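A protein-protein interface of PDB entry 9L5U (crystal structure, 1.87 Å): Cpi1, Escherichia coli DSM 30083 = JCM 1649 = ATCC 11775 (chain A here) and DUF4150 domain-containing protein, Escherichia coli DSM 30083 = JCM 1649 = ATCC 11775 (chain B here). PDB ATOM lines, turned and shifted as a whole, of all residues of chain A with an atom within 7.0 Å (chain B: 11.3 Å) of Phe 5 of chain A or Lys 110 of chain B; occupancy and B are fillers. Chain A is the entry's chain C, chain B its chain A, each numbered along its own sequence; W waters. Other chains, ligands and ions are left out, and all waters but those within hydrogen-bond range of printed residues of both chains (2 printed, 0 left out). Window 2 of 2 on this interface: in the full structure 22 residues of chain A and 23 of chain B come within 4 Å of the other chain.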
ATOM      1  N   GLY A   2      31.243  12.063   2.007  1.00  0.00           N
ATOM      2  CA  GLY A   2      31.370  11.767   3.423  1.00  0.00           C
ATOM      3  C   GLY A   2      32.753  11.260   3.796  1.00  0.00           C
ATOM      4  O   GLY A   2      33.558  10.946   2.910  1.00  0.00           O
ATOM      5  N   ILE A   3      33.024  11.187   5.104  1.00  0.00           N
ATOM      6  CA  ILE A   3      34.289  10.682   5.635  1.00  0.00           C
ATOM      7  C   ILE A   3      34.277   9.159   5.653  1.00  0.00           C
ATOM      8  O   ILE A   3      33.273   8.525   5.290  1.00  0.00           O
ATOM      9  CB  ILE A   3      34.551  11.217   7.051  1.00  0.00           C
ATOM     10  CG1 ILE A   3      33.470  10.708   8.015  1.00  0.00           C
ATOM     11  CG2 ILE A   3      34.610  12.715   7.043  1.00  0.00           C
ATOM     12  CD1 ILE A   3      34.019  10.223   9.368  1.00  0.00           C
ATOM     13  N   VAL A   4      35.370   8.567   6.128  1.00  0.00           N
ATOM     14  CA  VAL A   4      35.497   7.114   6.206  1.00  0.00           C
ATOM     15  C   VAL A   4      34.949   6.631   7.547  1.00  0.00           C
ATOM     16  O   VAL A   4      35.435   7.040   8.608  1.00  0.00           O
ATOM     17  CB  VAL A   4      36.957   6.675   6.029  1.00  0.00           C
ATOM     18  CG1 VAL A   4      37.061   5.159   6.176  1.00  0.00           C
ATOM     19  CG2 VAL A   4      37.503   7.136   4.669  1.00  0.00           C
ATOM     20  N   PHE A   5      33.948   5.748   7.502  1.00  0.00           N
ATOM     21  CA  PHE A   5      33.518   4.980   8.669  1.00  0.00           C
ATOM     22  C   PHE A   5      34.231   3.631   8.626  1.00  0.00           C
ATOM     23  O   PHE A   5      34.140   2.908   7.627  1.00  0.00           O
ATOM     24  CB  PHE A   5      31.999   4.796   8.694  1.00  0.00           C
ATOM     25  CG  PHE A   5      31.249   5.982   9.248  1.00  0.00           C
ATOM     26  CD1 PHE A   5      30.264   5.808  10.209  1.00  0.00           C
ATOM     27  CD2 PHE A   5      31.518   7.265   8.798  1.00  0.00           C
ATOM     28  CE1 PHE A   5      29.547   6.901  10.719  1.00  0.00           C
ATOM     29  CE2 PHE A   5      30.826   8.368   9.306  1.00  0.00           C
ATOM     30  CZ  PHE A   5      29.835   8.186  10.267  1.00  0.00           C
ATOM     31  N   THR A   6      34.980   3.317   9.681  1.00  0.00           N
ATOM     32  CA  THR A   6      35.730   2.065   9.721  1.00  0.00           C
ATOM     33  C   THR A   6      34.794   0.877   9.472  1.00  0.00           C
ATOM     34  O   THR A   6      33.737   0.777  10.093  1.00  0.00           O
ATOM     35  CB  THR A   6      36.417   1.918  11.083  1.00  0.00           C
ATOM     36  OG1 THR A   6      37.144   3.119  11.394  1.00  0.00           O
ATOM     37  CG2 THR A   6      37.358   0.704  11.097  1.00  0.00           C
ATOM     38  N   ASN A   7      35.172  -0.013   8.550  1.00  0.00           N
ATOM     39  CA  ASN A   7      34.303  -1.144   8.223  1.00  0.00           C
ATOM     40  C   ASN A   7      34.517  -2.298   9.210  1.00  0.00           C
ATOM     41  O   ASN A   7      35.541  -2.382   9.893  1.00  0.00           O
ATOM     42  CB  ASN A   7      34.528  -1.614   6.782  1.00  0.00           C
ATOM     43  CG  ASN A   7      35.933  -2.141   6.540  1.00  0.00           C
ATOM     44  OD1 ASN A   7      36.698  -2.388   7.476  1.00  0.00           O
ATOM     45  ND2 ASN A   7      36.281  -2.317   5.264  1.00  0.00           N
ATOM     46  N   HIS A   8      33.512  -3.176   9.300  1.00  0.00           N
ATOM     47  CA  HIS A   8      33.527  -4.283  10.256  1.00  0.00           C
ATOM     48  C   HIS A   8      32.862  -5.504   9.649  1.00  0.00           C
ATOM     49  O   HIS A   8      32.075  -5.399   8.705  1.00  0.00           O
ATOM     50  CB  HIS A   8      32.800  -3.930  11.571  1.00  0.00           C
ATOM     51  CG  HIS A   8      33.438  -2.804  12.307  1.00  0.00           C
ATOM     52  ND1 HIS A   8      34.499  -2.984  13.169  1.00  0.00           N
ATOM     53  CD2 HIS A   8      33.211  -1.470  12.254  1.00  0.00           C
ATOM     54  CE1 HIS A   8      34.887  -1.807  13.632  1.00  0.00           C
ATOM     55  NE2 HIS A   8      34.119  -0.873  13.095  1.00  0.00           N
ATOM     56  N   MET A  61      21.746   1.091  16.183  1.00  0.00           N
ATOM     57  CA  MET A  61      21.871   2.455  15.686  1.00  0.00           C
ATOM     58  C   MET A  61      23.318   2.796  15.330  1.00  0.00           C
ATOM     59  O   MET A  61      23.560   3.579  14.405  1.00  0.00           O
ATOM     60  CB  MET A  61      21.335   3.442  16.712  1.00  0.00           C
ATOM     61  CG  MET A  61      19.819   3.436  16.842  1.00  0.00           C
ATOM     62  SD  MET A  61      18.986   3.960  15.340  1.00  0.00           S
ATOM     63  CE  MET A  61      19.366   5.700  15.375  1.00  0.00           C
ATOM     64  N   SER A  62      24.289   2.225  16.037  1.00  0.00           N
ATOM     65  CA  SER A  62      25.682   2.535  15.743  1.00  0.00           C
ATOM     66  C   SER A  62      26.133   1.901  14.442  1.00  0.00           C
ATOM     67  O   SER A  62      27.079   2.393  13.813  1.00  0.00           O
ATOM     68  CB  SER A  62      26.577   2.094  16.912  1.00  0.00           C
ATOM     69  OG  SER A  62      26.760   0.696  16.921  1.00  0.00           O
ATOM     70  N   MET A  64      23.859   1.089  11.839  1.00  0.00           N
ATOM     71  CA  MET A  64      23.020   1.540  10.736  1.00  0.00           C
ATOM     72  C   MET A  64      23.795   2.350   9.704  1.00  0.00           C
ATOM     73  O   MET A  64      23.514   2.192   8.499  1.00  0.00           O
ATOM     74  CB  MET A  64      21.845   2.372  11.274  1.00  0.00           C
ATOM     75  CG  MET A  64      20.660   1.577  11.799  1.00  0.00           C
ATOM     76  SD  MET A  64      19.660   0.946  10.439  1.00  0.00           S
ATOM     77  CE  MET A  64      18.571  -0.140  11.358  1.00  0.00           C
ATOM     78  N   PRO A  65      24.743   3.224  10.078  1.00  0.00           N
ATOM     79  CA  PRO A  65      25.488   3.956   9.043  1.00  0.00           C
ATOM     80  C   PRO A  65      26.258   3.035   8.135  1.00  0.00           C
ATOM     81  O   PRO A  65      26.511   3.388   6.979  1.00  0.00           O
ATOM     82  CB  PRO A  65      26.427   4.867   9.849  1.00  0.00           C
ATOM     83  CG  PRO A  65      25.756   5.033  11.167  1.00  0.00           C
ATOM     84  CD  PRO A  65      25.071   3.698  11.435  1.00  0.00           C
ATOM     85  N   LEU A  66      26.628   1.853   8.625  1.00  0.00           N
ATOM     86  CA  LEU A  66      27.361   0.906   7.800  1.00  0.00           C
ATOM     87  C   LEU A  66      26.435   0.042   6.947  1.00  0.00           C
ATOM     88  O   LEU A  66      26.833  -0.393   5.861  1.00  0.00           O
ATOM     89  CB  LEU A  66      28.239   0.022   8.685  1.00  0.00           C
ATOM     90  CG  LEU A  66      29.205   0.750   9.625  1.00  0.00           C
ATOM     91  CD1 LEU A  66      29.858  -0.188  10.608  1.00  0.00           C
ATOM     92  CD2 LEU A  66      30.254   1.456   8.777  1.00  0.00           C
ATOM     93  N   GLY B  17      18.219  12.630   2.248  1.00  0.00           N
ATOM     94  CA  GLY B  17      16.830  12.850   1.881  1.00  0.00           C
ATOM     95  C   GLY B  17      16.552  12.567   0.416  1.00  0.00           C
ATOM     96  O   GLY B  17      15.658  13.177  -0.186  1.00  0.00           O
ATOM     97  N   ASN B  18      17.309  11.622  -0.147  1.00  0.00           N
ATOM     98  CA  ASN B  18      17.312  11.359  -1.580  1.00  0.00           C
ATOM     99  C   ASN B  18      16.205  10.413  -2.029  1.00  0.00           C
ATOM    100  O   ASN B  18      16.220   9.975  -3.187  1.00  0.00           O
ATOM    101  CB  ASN B  18      18.668  10.786  -2.011  1.00  0.00           C
ATOM    102  CG  ASN B  18      19.721  11.859  -2.217  1.00  0.00           C
ATOM    103  OD1 ASN B  18      19.878  12.760  -1.387  1.00  0.00           O
ATOM    104  ND2 ASN B  18      20.453  11.771  -3.328  1.00  0.00           N
ATOM    105  N   TRP B  19      15.258  10.074  -1.162  1.00  0.00           N
ATOM    106  CA  TRP B  19      14.255   9.113  -1.592  1.00  0.00           C
ATOM    107  C   TRP B  19      13.212   9.794  -2.476  1.00  0.00           C
ATOM    108  O   TRP B  19      13.106  11.018  -2.518  1.00  0.00           O
ATOM    109  CB  TRP B  19      13.609   8.432  -0.382  1.00  0.00           C
ATOM    110  CG  TRP B  19      13.020   9.353   0.654  1.00  0.00           C
ATOM    111  CD1 TRP B  19      11.774   9.910   0.635  1.00  0.00           C
ATOM    112  CD2 TRP B  19      13.633   9.777   1.879  1.00  0.00           C
ATOM    113  NE1 TRP B  19      11.577  10.668   1.768  1.00  0.00           N
ATOM    114  CE2 TRP B  19      12.703  10.602   2.548  1.00  0.00           C
ATOM    115  CE3 TRP B  19      14.877   9.543   2.472  1.00  0.00           C
ATOM    116  CZ2 TRP B  19      12.976  11.193   3.782  1.00  0.00           C
ATOM    117  CZ3 TRP B  19      15.148  10.130   3.697  1.00  0.00           C
ATOM    118  CH2 TRP B  19      14.194  10.944   4.343  1.00  0.00           C
ATOM    119  N   LEU B  36      19.285  19.404  13.273  1.00  0.00           N
ATOM    120  CA  LEU B  36      19.442  18.196  12.461  1.00  0.00           C
ATOM    121  C   LEU B  36      18.834  16.979  13.148  1.00  0.00           C
ATOM    122  O   LEU B  36      18.155  16.165  12.506  1.00  0.00           O
ATOM    123  CB  LEU B  36      20.924  17.960  12.154  1.00  0.00           C
ATOM    124  CG  LEU B  36      21.337  16.702  11.378  1.00  0.00           C
ATOM    125  CD1 LEU B  36      22.522  17.010  10.470  1.00  0.00           C
ATOM    126  CD2 LEU B  36      21.669  15.531  12.311  1.00  0.00           C
ATOM    127  N   THR B  37      19.056  16.835  14.454  1.00  0.00           N
ATOM    128  CA  THR B  37      18.545  15.670  15.155  1.00  0.00           C
ATOM    129  C   THR B  37      17.095  15.829  15.569  1.00  0.00           C
ATOM    130  O   THR B  37      16.502  14.871  16.082  1.00  0.00           O
ATOM    131  CB  THR B  37      19.399  15.401  16.391  1.00  0.00           C
ATOM    132  OG1 THR B  37      19.417  16.580  17.200  1.00  0.00           O
ATOM    133  CG2 THR B  37      20.816  15.065  15.973  1.00  0.00           C
ATOM    134  N   CYS B  39      14.310  15.803  14.194  1.00  0.00           N
ATOM    135  CA  CYS B  39      13.127  15.300  13.515  1.00  0.00           C
ATOM    136  C   CYS B  39      12.358  14.312  14.428  1.00  0.00           C
ATOM    137  O   CYS B  39      11.128  14.292  14.416  1.00  0.00           O
ATOM    138  CB  CYS B  39      13.489  14.685  12.176  1.00  0.00           C
ATOM    139  SG  CYS B  39      14.806  13.394  12.589  1.00  0.00           S
ATOM    140  N   THR B  65      17.037  10.363  19.147  1.00  0.00           N
ATOM    141  CA  THR B  65      17.118   9.751  17.833  1.00  0.00           C
ATOM    142  C   THR B  65      16.697   8.292  17.828  1.00  0.00           C
ATOM    143  O   THR B  65      16.149   7.854  16.831  1.00  0.00           O
ATOM    144  CB  THR B  65      18.546   9.833  17.257  1.00  0.00           C
ATOM    145  OG1 THR B  65      19.436   9.169  18.158  1.00  0.00           O
ATOM    146  CG2 THR B  65      19.015  11.278  17.081  1.00  0.00           C
ATOM    147  N   MET B 103      11.336   5.674  10.921  1.00  0.00           N
ATOM    148  CA  MET B 103      12.711   6.114  10.704  1.00  0.00           C
ATOM    149  C   MET B 103      13.126   5.791   9.275  1.00  0.00           C
ATOM    150  O   MET B 103      13.219   4.620   8.901  1.00  0.00           O
ATOM    151  CB  MET B 103      13.682   5.464  11.695  1.00  0.00           C
ATOM    152  CG  MET B 103      15.100   6.114  11.597  1.00  0.00           C
ATOM    153  SD  MET B 103      16.346   5.321  12.631  1.00  0.00           S
ATOM    154  CE  MET B 103      15.682   5.605  14.273  1.00  0.00           C
ATOM    155  N   MET B 104      13.382   6.832   8.490  1.00  0.00           N
ATOM    156  CA  MET B 104      13.849   6.705   7.121  1.00  0.00           C
ATOM    157  C   MET B 104      15.370   6.663   7.115  1.00  0.00           C
ATOM    158  O   MET B 104      16.023   7.466   7.786  1.00  0.00           O
ATOM    159  CB  MET B 104      13.353   7.888   6.286  1.00  0.00           C
ATOM    160  CG  MET B 104      11.856   8.163   6.425  1.00  0.00           C
ATOM    161  SD  MET B 104      10.855   6.727   5.861  1.00  0.00           S
ATOM    162  CE  MET B 104      10.614   7.167   4.138  1.00  0.00           C
ATOM    163  N   TRP B 105      15.948   5.733   6.373  1.00  0.00           N
ATOM    164  CA  TRP B 105      17.412   5.666   6.351  1.00  0.00           C
ATOM    165  C   TRP B 105      17.827   5.253   4.943  1.00  0.00           C
ATOM    166  O   TRP B 105      17.856   4.070   4.626  1.00  0.00           O
ATOM    167  CB  TRP B 105      17.945   4.713   7.418  1.00  0.00           C
ATOM    168  CG  TRP B 105      19.358   5.029   7.768  1.00  0.00           C
ATOM    169  CD1 TRP B 105      20.402   5.218   6.887  1.00  0.00           C
ATOM    170  CD2 TRP B 105      19.898   5.221   9.082  1.00  0.00           C
ATOM    171  NE1 TRP B 105      21.556   5.520   7.587  1.00  0.00           N
ATOM    172  CE2 TRP B 105      21.274   5.532   8.929  1.00  0.00           C
ATOM    173  CE3 TRP B 105      19.351   5.181  10.368  1.00  0.00           C
ATOM    174  CZ2 TRP B 105      22.114   5.792  10.030  1.00  0.00           C
ATOM    175  CZ3 TRP B 105      20.176   5.432  11.460  1.00  0.00           C
ATOM    176  CH2 TRP B 105      21.551   5.736  11.282  1.00  0.00           C
ATOM    177  N   ASP B 106      18.140   6.230   4.109  1.00  0.00           N
ATOM    178  CA  ASP B 106      18.436   5.951   2.708  1.00  0.00           C
ATOM    179  C   ASP B 106      19.909   5.587   2.524  1.00  0.00           C
ATOM    180  O   ASP B 106      20.753   5.805   3.405  1.00  0.00           O
ATOM    181  CB  ASP B 106      18.074   7.143   1.819  1.00  0.00           C
ATOM    182  CG  ASP B 106      18.912   8.368   2.111  1.00  0.00           C
ATOM    183  OD1 ASP B 106      18.704   8.992   3.174  1.00  0.00           O
ATOM    184  OD2 ASP B 106      19.781   8.708   1.276  1.00  0.00           O
ATOM    185  N   SER B 107      20.203   5.010   1.357  1.00  0.00           N
ATOM    186  CA  SER B 107      21.547   4.541   1.048  1.00  0.00           C
ATOM    187  C   SER B 107      22.531   5.688   1.130  1.00  0.00           C
ATOM    188  O   SER B 107      22.256   6.802   0.669  1.00  0.00           O
ATOM    189  CB  SER B 107      21.595   3.941  -0.355  1.00  0.00           C
ATOM    190  OG  SER B 107      21.133   4.893  -1.299  1.00  0.00           O
ATOM    191  N   GLY B 108      23.689   5.417   1.717  1.00  0.00           N
ATOM    192  CA  GLY B 108      24.707   6.429   1.835  1.00  0.00           C
ATOM    193  C   GLY B 108      24.540   7.374   3.002  1.00  0.00           C
ATOM    194  O   GLY B 108      25.498   8.071   3.351  1.00  0.00           O
ATOM    195  N   SER B 109      23.371   7.425   3.635  1.00  0.00           N
ATOM    196  CA  SER B 109      23.196   8.347   4.751  1.00  0.00           C
ATOM    197  C   SER B 109      23.889   7.815   6.003  1.00  0.00           C
ATOM    198  O   SER B 109      23.877   6.614   6.281  1.00  0.00           O
ATOM    199  CB  SER B 109      21.714   8.586   5.056  1.00  0.00           C
ATOM    200  OG  SER B 109      21.573   9.525   6.127  1.00  0.00           O
ATOM    201  N   LYS B 110      24.484   8.721   6.763  1.00  0.00           N
ATOM    202  CA  LYS B 110      25.045   8.384   8.062  1.00  0.00           C
ATOM    203  C   LYS B 110      24.058   8.595   9.193  1.00  0.00           C
ATOM    204  O   LYS B 110      24.395   8.301  10.349  1.00  0.00           O
ATOM    205  CB  LYS B 110      26.319   9.212   8.316  1.00  0.00           C
ATOM    206  CG  LYS B 110      27.402   9.063   7.239  1.00  0.00           C
ATOM    207  CD  LYS B 110      27.750   7.608   6.948  1.00  0.00           C
ATOM    208  CE  LYS B 110      28.746   7.470   5.769  1.00  0.00           C
ATOM    209  NZ  LYS B 110      28.226   6.689   4.587  1.00  0.00           N
ATOM    210  N   VAL B 111      22.847   9.088   8.896  1.00  0.00           N
ATOM    211  CA  VAL B 111      21.854   9.349   9.932  1.00  0.00           C
ATOM    212  C   VAL B 111      20.486   8.908   9.443  1.00  0.00           C
ATOM    213  O   VAL B 111      20.207   8.897   8.238  1.00  0.00           O
ATOM    214  CB  VAL B 111      21.807  10.846  10.335  1.00  0.00           C
ATOM    215  CG1 VAL B 111      23.070  11.237  11.088  1.00  0.00           C
ATOM    216  CG2 VAL B 111      21.628  11.719   9.091  1.00  0.00           C
ATOM    217  N   GLY B 112      19.641   8.540  10.400  1.00  0.00           N
ATOM    218  CA  GLY B 112      18.237   8.308  10.140  1.00  0.00           C
ATOM    219  C   GLY B 112      17.466   9.604  10.182  1.00  0.00           C
ATOM    220  O   GLY B 112      17.975  10.638  10.613  1.00  0.00           O
ATOM    221  N   HIS B 113      16.242   9.564   9.668  1.00  0.00           N
ATOM    222  CA  HIS B 113      15.395  10.755   9.608  1.00  0.00           C
ATOM    223  C   HIS B 113      13.973  10.308   9.919  1.00  0.00           C
ATOM    224  O   HIS B 113      13.367   9.546   9.153  1.00  0.00           O
ATOM    225  CB  HIS B 113      15.480  11.448   8.234  1.00  0.00           C
ATOM    226  CG  HIS B 113      14.585  12.645   8.130  1.00  0.00           C
ATOM    227  ND1 HIS B 113      14.784  13.786   8.882  1.00  0.00           N
ATOM    228  CD2 HIS B 113      13.452  12.857   7.418  1.00  0.00           C
ATOM    229  CE1 HIS B 113      13.825  14.656   8.620  1.00  0.00           C
ATOM    230  NE2 HIS B 113      13.001  14.116   7.738  1.00  0.00           N
ATOM    231  N   TRP B 114      13.445  10.764  11.050  1.00  0.00           N
ATOM    232  CA  TRP B 114      12.081  10.424  11.442  1.00  0.00           C
ATOM    233  C   TRP B 114      11.077  11.209  10.605  1.00  0.00           C
ATOM    234  O   TRP B 114      11.221  12.426  10.432  1.00  0.00           O
ATOM    235  CB  TRP B 114      11.861  10.738  12.925  1.00  0.00           C
ATOM    236  CG  TRP B 114      12.519   9.753  13.855  1.00  0.00           C
ATOM    237  CD1 TRP B 114      13.687   9.910  14.535  1.00  0.00           C
ATOM    238  CD2 TRP B 114      12.017   8.460  14.212  1.00  0.00           C
ATOM    239  NE1 TRP B 114      13.951   8.792  15.292  1.00  0.00           N
ATOM    240  CE2 TRP B 114      12.942   7.885  15.105  1.00  0.00           C
ATOM    241  CE3 TRP B 114      10.889   7.727  13.833  1.00  0.00           C
ATOM    242  CZ2 TRP B 114      12.764   6.607  15.651  1.00  0.00           C
ATOM    243  CZ3 TRP B 114      10.711   6.457  14.371  1.00  0.00           C
ATOM    244  CH2 TRP B 114      11.649   5.906  15.266  1.00  0.00           C
ATOM    245  N   ASN B 149      13.600   1.989   7.601  1.00  0.00           N
ATOM    246  CA  ASN B 149      14.497   0.919   8.038  1.00  0.00           C
ATOM    247  C   ASN B 149      13.820  -0.054   8.997  1.00  0.00           C
ATOM    248  O   ASN B 149      14.491  -0.928   9.556  1.00  0.00           O
ATOM    249  CB  ASN B 149      15.799   1.503   8.651  1.00  0.00           C
ATOM    250  CG  ASN B 149      15.589   2.177  10.007  1.00  0.00           C
ATOM    251  OD1 ASN B 149      14.489   2.215  10.532  1.00  0.00           O
ATOM    252  ND2 ASN B 149      16.675   2.688  10.591  1.00  0.00           N
HETATM  253  O   HOH W   1      25.005   4.453   5.026  1.00  0.00           O
HETATM  254  O   HOH W   2      29.274   3.882   5.677  1.00  0.00           O
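ND2 of Asn 149 of chain B is in hydrogen-bond range of SD of Met 64 of chain A, 3.5 Å away.
O of Met 103 of chain B lies within hydrogen-bond range of N of Asn 149 of chain B (3.0 Å).
The indole nitrogen (NE1) of Trp 105 of chain B sits at hydrogen-bond distance from the backbone carbonyl oxygen (O) of Ser 109 of chain B, 2.9 Å away.
O of Gly 108 of chain B sits at hydrogen-bond distance from NZ of Lys 110 of chain B, 3.3 Å away.
Phe 5 of chain A touches Lys 110 of chain B.
SD of Met 61 of chain A touches CE of Met 103 of chain B, at 3.8 Å.
Met 64 of chain A touches Trp 105 of chain B (CB to CH2, 3.4 Å).
Trp 105 of chain B touches Pro 65 of chain A (CZ2 to N, 3.7 Å).
Lys 110 of chain B touches Pro 65 of chain A.
No residue of chain B comes within 4 Å of Gly 2 of chain A.
No residue of chain B comes within 4 Å of Val 4 of chain A.
Phe 5 of chain A touches one residue of chain B.
No residue of chain B comes within 4 Å of Thr 6 of chain A.
No residue of chain B comes within 4 Å of Asn 7 of chain A.
Of the printed residues of chain B, Met 61 of chain A touches Met 103.
Of the printed residues of chain B, Met 64 of chain A touches Trp 105 (3.4 Å) and Asn 149 (3.5 Å).
Of the printed residues of chain A, Trp 105 of chain B touches Met 64 (3.4 Å) and Pro 65 (3.7 Å).
Lys 110 of chain B touches just these residues of chain A: Phe 5 (3.9 Å) and Pro 65 (3.6 Å).
Printed residues of chain A within 4 Å of Asn 149 of chain B: Met 64.
The nearest printed residue of chain B that does not touch Phe 5 of chain A is Val 111 of chain B (7.2 Å).
The nearest printed residue of chain B that does not touch Met 64 of chain A is Ser 109 of chain B (5.0 Å).
Of the 20 printed residues of chain B, 4 touch a printed residue of chain A.
Along chain B the printed residues that touch a printed residue of chain A span positions 103 to 149.
Hydrophobic or aromatic side chains of chain A within 4 Å of the printed part of chain B: Phe 5, Met 61, Met 64 and Pro 65.
Among the printed residues, 6 pairs touch across the chains.
Among the printed residues, no Asp or Glu carboxylate lies within 4 Å of a Lys or Arg side-chain nitrogen of the other chain.
Water W1 bridges the backbone carbonyl oxygen (O) of Pro 65 of chain A (2.7 Å) and the backbone carbonyl oxygen (O) of Ser 109 of chain B (2.7 Å).
Water W2 lies within hydrogen-bond range of O of Pro 65 of chain A and NZ of Lys 110 of chain B.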
